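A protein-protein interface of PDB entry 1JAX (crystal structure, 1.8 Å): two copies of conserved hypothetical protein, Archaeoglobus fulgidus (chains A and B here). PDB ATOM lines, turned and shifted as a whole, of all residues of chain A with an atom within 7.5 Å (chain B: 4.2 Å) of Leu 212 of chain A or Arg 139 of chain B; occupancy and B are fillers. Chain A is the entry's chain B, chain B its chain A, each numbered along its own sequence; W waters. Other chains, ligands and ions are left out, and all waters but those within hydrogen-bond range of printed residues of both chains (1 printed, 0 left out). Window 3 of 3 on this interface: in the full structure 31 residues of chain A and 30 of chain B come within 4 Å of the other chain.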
ATOM      1  N   ASP A 148     -35.013  -9.635 -12.566  1.00  0.00           N
ATOM      2  CA  ASP A 148     -33.892  -8.763 -12.226  1.00  0.00           C
ATOM      3  C   ASP A 148     -33.385  -9.279 -10.887  1.00  0.00           C
ATOM      4  O   ASP A 148     -33.821  -8.824  -9.817  1.00  0.00           O
ATOM      5  CB  ASP A 148     -34.359  -7.316 -12.084  1.00  0.00           C
ATOM      6  CG  ASP A 148     -33.220  -6.372 -11.790  1.00  0.00           C
ATOM      7  OD1 ASP A 148     -33.496  -5.186 -11.516  1.00  0.00           O
ATOM      8  OD2 ASP A 148     -32.048  -6.815 -11.828  1.00  0.00           O
ATOM      9  N   ASP A 150     -30.032 -10.690  -8.317  1.00  0.00           N
ATOM     10  CA  ASP A 150     -28.597 -10.654  -8.036  1.00  0.00           C
ATOM     11  C   ASP A 150     -28.132 -12.065  -7.657  1.00  0.00           C
ATOM     12  O   ASP A 150     -28.877 -12.867  -7.061  1.00  0.00           O
ATOM     13  CB  ASP A 150     -28.280  -9.666  -6.895  1.00  0.00           C
ATOM     14  CG  ASP A 150     -28.326  -8.230  -7.346  1.00  0.00           C
ATOM     15  OD1 ASP A 150     -28.301  -7.970  -8.577  1.00  0.00           O
ATOM     16  OD2 ASP A 150     -28.366  -7.346  -6.463  1.00  0.00           O
ATOM     17  N   ARG A 175     -27.309 -10.523 -12.218  1.00  0.00           N
ATOM     18  CA  ARG A 175     -26.143  -9.696 -11.948  1.00  0.00           C
ATOM     19  C   ARG A 175     -25.320 -10.398 -10.892  1.00  0.00           C
ATOM     20  O   ARG A 175     -25.760 -10.522  -9.754  1.00  0.00           O
ATOM     21  CB  ARG A 175     -26.535  -8.322 -11.401  1.00  0.00           C
ATOM     22  CG  ARG A 175     -25.274  -7.499 -11.041  1.00  0.00           C
ATOM     23  CD  ARG A 175     -25.577  -6.060 -10.596  1.00  0.00           C
ATOM     24  NE  ARG A 175     -26.384  -6.000  -9.374  1.00  0.00           N
ATOM     25  CZ  ARG A 175     -26.425  -4.944  -8.566  1.00  0.00           C
ATOM     26  NH1 ARG A 175     -25.703  -3.861  -8.842  1.00  0.00           N
ATOM     27  NH2 ARG A 175     -27.182  -4.961  -7.481  1.00  0.00           N
ATOM     28  N   LEU A 177     -22.436 -10.864  -8.074  1.00  0.00           N
ATOM     29  CA  LEU A 177     -21.768  -9.992  -7.108  1.00  0.00           C
ATOM     30  C   LEU A 177     -20.771 -10.833  -6.343  1.00  0.00           C
ATOM     31  O   LEU A 177     -21.118 -11.865  -5.805  1.00  0.00           O
ATOM     32  CB  LEU A 177     -22.767  -9.393  -6.102  1.00  0.00           C
ATOM     33  CG  LEU A 177     -23.800  -8.410  -6.659  1.00  0.00           C
ATOM     34  CD1 LEU A 177     -24.847  -8.100  -5.594  1.00  0.00           C
ATOM     35  CD2 LEU A 177     -23.104  -7.138  -7.092  1.00  0.00           C
ATOM     36  N   LYS A 210     -32.426  -8.846  -4.615  1.00  0.00           N
ATOM     37  CA  LYS A 210     -31.728  -7.741  -5.264  1.00  0.00           C
ATOM     38  C   LYS A 210     -31.109  -6.901  -4.153  1.00  0.00           C
ATOM     39  O   LYS A 210     -31.764  -6.622  -3.148  1.00  0.00           O
ATOM     40  CB  LYS A 210     -32.715  -6.870  -6.055  1.00  0.00           C
ATOM     41  CG  LYS A 210     -32.067  -5.830  -6.949  1.00  0.00           C
ATOM     42  CD  LYS A 210     -31.420  -6.480  -8.167  1.00  0.00           C
ATOM     43  CE  LYS A 210     -30.665  -5.469  -8.995  1.00  0.00           C
ATOM     44  NZ  LYS A 210     -29.977  -6.163 -10.095  1.00  0.00           N
ATOM     45  N   PHE A 211     -29.851  -6.502  -4.322  1.00  0.00           N
ATOM     46  CA  PHE A 211     -29.181  -5.652  -3.336  1.00  0.00           C
ATOM     47  C   PHE A 211     -29.127  -4.269  -3.965  1.00  0.00           C
ATOM     48  O   PHE A 211     -28.560  -4.088  -5.036  1.00  0.00           O
ATOM     49  CB  PHE A 211     -27.778  -6.192  -3.048  1.00  0.00           C
ATOM     50  CG  PHE A 211     -27.791  -7.559  -2.441  1.00  0.00           C
ATOM     51  CD1 PHE A 211     -27.717  -8.699  -3.233  1.00  0.00           C
ATOM     52  CD2 PHE A 211     -27.933  -7.710  -1.056  1.00  0.00           C
ATOM     53  CE1 PHE A 211     -27.782  -9.977  -2.653  1.00  0.00           C
ATOM     54  CE2 PHE A 211     -27.999  -8.977  -0.478  1.00  0.00           C
ATOM     55  CZ  PHE A 211     -27.922 -10.110  -1.278  1.00  0.00           C
ATOM     56  N   LEU A 212     -29.699  -3.276  -3.296  1.00  0.00           N
ATOM     57  CA  LEU A 212     -29.703  -1.917  -3.834  1.00  0.00           C
ATOM     58  C   LEU A 212     -29.871  -0.881  -2.739  1.00  0.00           C
ATOM     59  O   LEU A 212     -29.602   0.310  -3.016  1.00  0.00           O
ATOM     60  CB  LEU A 212     -30.822  -1.745  -4.867  1.00  0.00           C
ATOM     61  CG  LEU A 212     -30.614  -2.175  -6.321  1.00  0.00           C
ATOM     62  CD1 LEU A 212     -31.721  -1.535  -7.178  1.00  0.00           C
ATOM     63  CD2 LEU A 212     -29.230  -1.710  -6.827  1.00  0.00           C
ATOM     64  OXT LEU A 212     -30.278  -1.268  -1.629  1.00  0.00           O
ATOM     65  N   PRO B 136     -29.621   0.557   5.443  1.00  0.00           N
ATOM     66  CA  PRO B 136     -28.412   1.395   5.354  1.00  0.00           C
ATOM     67  C   PRO B 136     -28.721   2.669   6.141  1.00  0.00           C
ATOM     68  O   PRO B 136     -29.549   3.487   5.719  1.00  0.00           O
ATOM     69  CB  PRO B 136     -28.297   1.674   3.862  1.00  0.00           C
ATOM     70  CG  PRO B 136     -28.809   0.432   3.255  1.00  0.00           C
ATOM     71  CD  PRO B 136     -30.019   0.075   4.112  1.00  0.00           C
ATOM     72  N   ALA B 137     -28.024   2.842   7.260  1.00  0.00           N
ATOM     73  CA  ALA B 137     -28.244   3.955   8.169  1.00  0.00           C
ATOM     74  C   ALA B 137     -28.169   5.362   7.602  1.00  0.00           C
ATOM     75  O   ALA B 137     -29.111   6.131   7.749  1.00  0.00           O
ATOM     76  CB  ALA B 137     -27.292   3.833   9.347  1.00  0.00           C
ATOM     77  N   ALA B 138     -27.045   5.710   6.983  1.00  0.00           N
ATOM     78  CA  ALA B 138     -26.873   7.050   6.434  1.00  0.00           C
ATOM     79  C   ALA B 138     -27.894   7.364   5.350  1.00  0.00           C
ATOM     80  O   ALA B 138     -28.430   8.478   5.292  1.00  0.00           O
ATOM     81  CB  ALA B 138     -25.453   7.218   5.881  1.00  0.00           C
ATOM     82  N   ARG B 139     -28.169   6.391   4.485  1.00  0.00           N
ATOM     83  CA  ARG B 139     -29.135   6.617   3.423  1.00  0.00           C
ATOM     84  C   ARG B 139     -30.525   6.830   4.004  1.00  0.00           C
ATOM     85  O   ARG B 139     -31.257   7.716   3.564  1.00  0.00           O
ATOM     86  CB  ARG B 139     -29.148   5.424   2.458  1.00  0.00           C
ATOM     87  CG  ARG B 139     -27.844   5.311   1.636  1.00  0.00           C
ATOM     88  CD  ARG B 139     -27.883   4.133   0.691  1.00  0.00           C
ATOM     89  NE  ARG B 139     -28.941   4.281  -0.299  1.00  0.00           N
ATOM     90  CZ  ARG B 139     -29.380   3.285  -1.064  1.00  0.00           C
ATOM     91  NH1 ARG B 139     -28.846   2.079  -0.950  1.00  0.00           N
ATOM     92  NH2 ARG B 139     -30.362   3.489  -1.932  1.00  0.00           N
ATOM     93  N   PHE B 140     -30.864   6.019   5.004  1.00  0.00           N
ATOM     94  CA  PHE B 140     -32.170   6.068   5.644  1.00  0.00           C
ATOM     95  C   PHE B 140     -32.389   7.371   6.409  1.00  0.00           C
ATOM     96  O   PHE B 140     -33.531   7.810   6.595  1.00  0.00           O
ATOM     97  CB  PHE B 140     -32.335   4.877   6.599  1.00  0.00           C
ATOM     98  CG  PHE B 140     -33.752   4.657   7.086  1.00  0.00           C
ATOM     99  CD1 PHE B 140     -34.781   4.356   6.188  1.00  0.00           C
ATOM    100  CD2 PHE B 140     -34.034   4.650   8.455  1.00  0.00           C
ATOM    101  CE1 PHE B 140     -36.076   4.037   6.647  1.00  0.00           C
ATOM    102  CE2 PHE B 140     -35.329   4.335   8.935  1.00  0.00           C
ATOM    103  CZ  PHE B 140     -36.351   4.027   8.031  1.00  0.00           C
ATOM    104  N   ALA B 141     -31.299   7.978   6.875  1.00  0.00           N
ATOM    105  CA  ALA B 141     -31.420   9.226   7.609  1.00  0.00           C
ATOM    106  C   ALA B 141     -31.632  10.436   6.699  1.00  0.00           C
ATOM    107  O   ALA B 141     -31.942  11.538   7.191  1.00  0.00           O
ATOM    108  CB  ALA B 141     -30.180   9.430   8.478  1.00  0.00           C
ATOM    109  N   ASN B 142     -31.463  10.247   5.394  1.00  0.00           N
ATOM    110  CA  ASN B 142     -31.641  11.325   4.405  1.00  0.00           C
ATOM    111  C   ASN B 142     -33.075  11.249   3.842  1.00  0.00           C
ATOM    112  O   ASN B 142     -33.415  10.302   3.153  1.00  0.00           O
ATOM    113  CB  ASN B 142     -30.607  11.164   3.271  1.00  0.00           C
ATOM    114  CG  ASN B 142     -30.936  12.003   2.040  1.00  0.00           C
ATOM    115  OD1 ASN B 142     -31.450  13.108   2.146  1.00  0.00           O
ATOM    116  ND2 ASN B 142     -30.629  11.468   0.861  1.00  0.00           N
ATOM    117  N   GLU B 145     -33.671  10.537   0.124  1.00  0.00           N
ATOM    118  CA  GLU B 145     -33.175   9.269  -0.416  1.00  0.00           C
ATOM    119  C   GLU B 145     -34.253   8.401  -1.025  1.00  0.00           C
ATOM    120  O   GLU B 145     -35.271   8.151  -0.389  1.00  0.00           O
ATOM    121  CB  GLU B 145     -32.495   8.454   0.689  1.00  0.00           C
ATOM    122  CG  GLU B 145     -31.712   7.226   0.218  1.00  0.00           C
ATOM    123  CD  GLU B 145     -30.366   7.589  -0.410  1.00  0.00           C
ATOM    124  OE1 GLU B 145     -29.842   8.677  -0.085  1.00  0.00           O
ATOM    125  OE2 GLU B 145     -29.832   6.786  -1.211  1.00  0.00           O
ATOM    126  N   LYS B 146     -34.031   7.928  -2.248  1.00  0.00           N
ATOM    127  CA  LYS B 146     -34.990   7.013  -2.859  1.00  0.00           C
ATOM    128  C   LYS B 146     -34.530   5.583  -2.566  1.00  0.00           C
ATOM    129  O   LYS B 146     -33.362   5.249  -2.749  1.00  0.00           O
ATOM    130  CB  LYS B 146     -35.036   7.205  -4.365  1.00  0.00           C
ATOM    131  CG  LYS B 146     -35.541   8.562  -4.779  1.00  0.00           C
ATOM    132  CD  LYS B 146     -35.595   8.633  -6.305  1.00  0.00           C
ATOM    133  CE  LYS B 146     -36.205   9.941  -6.758  1.00  0.00           C
ATOM    134  NZ  LYS B 146     -36.278   9.922  -8.247  1.00  0.00           N
ATOM    135  N   TRP B 149     -36.969  -1.051  -0.081  1.00  0.00           N
ATOM    136  CA  TRP B 149     -36.375  -2.145   0.688  1.00  0.00           C
ATOM    137  C   TRP B 149     -37.382  -3.018   1.427  1.00  0.00           C
ATOM    138  O   TRP B 149     -38.449  -2.541   1.873  1.00  0.00           O
ATOM    139  CB  TRP B 149     -35.388  -1.599   1.727  1.00  0.00           C
ATOM    140  CG  TRP B 149     -34.223  -0.850   1.176  1.00  0.00           C
ATOM    141  CD1 TRP B 149     -33.482  -1.166   0.073  1.00  0.00           C
ATOM    142  CD2 TRP B 149     -33.616   0.304   1.759  1.00  0.00           C
ATOM    143  NE1 TRP B 149     -32.441  -0.273  -0.065  1.00  0.00           N
ATOM    144  CE2 TRP B 149     -32.500   0.638   0.959  1.00  0.00           C
ATOM    145  CE3 TRP B 149     -33.912   1.089   2.885  1.00  0.00           C
ATOM    146  CZ2 TRP B 149     -31.670   1.725   1.253  1.00  0.00           C
ATOM    147  CZ3 TRP B 149     -33.077   2.179   3.184  1.00  0.00           C
ATOM    148  CH2 TRP B 149     -31.975   2.477   2.367  1.00  0.00           C
ATOM    149  N   GLU B 206     -23.365   1.311   0.904  1.00  0.00           N
ATOM    150  CA  GLU B 206     -24.299   0.525   1.707  1.00  0.00           C
ATOM    151  C   GLU B 206     -25.550   0.198   0.918  1.00  0.00           C
ATOM    152  O   GLU B 206     -26.064   1.014   0.156  1.00  0.00           O
ATOM    153  CB  GLU B 206     -24.637   1.227   3.038  1.00  0.00           C
ATOM    154  CG  GLU B 206     -23.517   1.078   4.078  1.00  0.00           C
ATOM    155  CD  GLU B 206     -23.853   1.641   5.452  1.00  0.00           C
ATOM    156  OE1 GLU B 206     -22.951   1.640   6.320  1.00  0.00           O
ATOM    157  OE2 GLU B 206     -25.003   2.080   5.672  1.00  0.00           O
ATOM    158  N   LEU B 207     -26.022  -1.020   1.124  1.00  0.00           N
ATOM    159  CA  LEU B 207     -27.174  -1.558   0.408  1.00  0.00           C
ATOM    160  C   LEU B 207     -28.207  -2.171   1.321  1.00  0.00           C
ATOM    161  O   LEU B 207     -27.902  -2.586   2.437  1.00  0.00           O
ATOM    162  CB  LEU B 207     -26.689  -2.682  -0.516  1.00  0.00           C
ATOM    163  CG  LEU B 207     -25.471  -2.350  -1.377  1.00  0.00           C
ATOM    164  CD1 LEU B 207     -24.852  -3.626  -1.961  1.00  0.00           C
ATOM    165  CD2 LEU B 207     -25.923  -1.389  -2.461  1.00  0.00           C
ATOM    166  N   GLY B 208     -29.423  -2.249   0.788  1.00  0.00           N
ATOM    167  CA  GLY B 208     -30.527  -2.885   1.459  1.00  0.00           C
ATOM    168  C   GLY B 208     -30.874  -4.107   0.618  1.00  0.00           C
ATOM    169  O   GLY B 208     -30.173  -4.425  -0.355  1.00  0.00           O
HETATM  170  O   HOH W   1     -32.527  -3.645  -2.419  1.00  0.00           O
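Of the 7 printed residues of chain A, 3 touch a printed residue of chain B.
Along chain A the printed residues that touch a printed residue of chain B span positions 210 to 212.
Printed residues of chain B that touch a printed residue of chain A: Arg 139, Trp 149, Leu 207 and Gly 208.
Hydrophobic or aromatic side chains of chain B within 4 Å of the printed part of chain A: Trp 149 and Leu 207.
Among the printed residues, no Asp or Glu carboxylate lies within 4 Å of a Lys or Arg side-chain nitrogen of the other chain.
Water W1 lies within hydrogen-bond range of the backbone NH (N) of Leu 212 of chain A, the backbone carbonyl oxygen (O) of Lys 210 of chain A and the backbone carbonyl oxygen (O) of Gly 208 of chain B.
Among the printed residues, merely in contact across the chains: Lys 210 of chain A with Gly 208 of chain B, Phe 211 of chain A with Gly 208 of chain B and Leu 212 of chain A with Leu 207 of chain B.
No position is printed for both chains.
Of the 6 pairs that touch across the chains among the printed residues, none has its exchanged pair printed and touching as well.
N of Gly 208 of chain B sits at hydrogen-bond distance from OXT of Leu 212 of chain A, 2.7 Å away.
NH1 of Arg 139 of chain B lies within salt-bridge range of O of Leu 212 of chain A (2.8 Å).
The indole nitrogen (NE1) of Trp 149 of chain B sits at hydrogen-bond distance from the chain-end carboxylate (OXT) of Leu 212 of chain A, 2.8 Å away.
Of chain B, only Arg 139 (2.8 Å), Trp 149 (2.8 Å), Leu 207 (3.7 Å) and Gly 208 (2.7 Å) come within 4 Å of Leu 212 of chain A.
No residue of chain A comes within 4 Å of Ala 138 of chain B.
Printed residues of chain B within 4 Å of Phe 211 of chain A: Gly 208 (3.4 Å).
Printed residues of chain B within 4 Å of Lys 210 of chain A: Gly 208 (3.9 Å).
Of the printed residues of chain A, Trp 149 of chain B touches Leu 212.
Of the printed residues of chain A, Leu 207 of chain B touches Leu 212 (3.7 Å).
Printed residues of chain A within 4 Å of Gly 208 of chain B: Lys 210 (3.9 Å), Phe 211 (3.4 Å) and Leu 212 (2.7 Å).
Leu 177 of chain A touches none of the printed residues of chain B.
The nearest residue of chain A that does not touch Arg 139 of chain B is Phe 211 of chain A (7.0 Å).
The nearest printed residue of chain B that does not touch Phe 211 of chain A is Leu 207 of chain B (4.04 Å).
OD1 of Asp 150 of chain A is in salt-bridge range of NZ of Lys 210 of chain A, at 2.9 Å.
NH1 of Arg 139 of chain B lies within hydrogen-bond range of O of Glu 206 of chain B (3.2 Å).
The side-chain carboxylate (OD2) of Asp 150 of chain A is in hydrogen-bond range of the backbone NH (N) of Phe 211 of chain A (2.7 Å).
The guanidinium group (NH2) of Arg 175 of chain A is in hydrogen-bond range of the backbone carbonyl oxygen (O) of Phe 211 of chain A (2.9 Å).
The guanidinium group (NE) of Arg 139 of chain B is in salt-bridge range of the side-chain carboxylate (OE2) of Glu 145 of chain B (2.8 Å).
The side-chain amino group (NZ) of Lys 210 of chain A is in salt-bridge range of the side-chain carboxylate (OD2) of Asp 148 of chain A.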
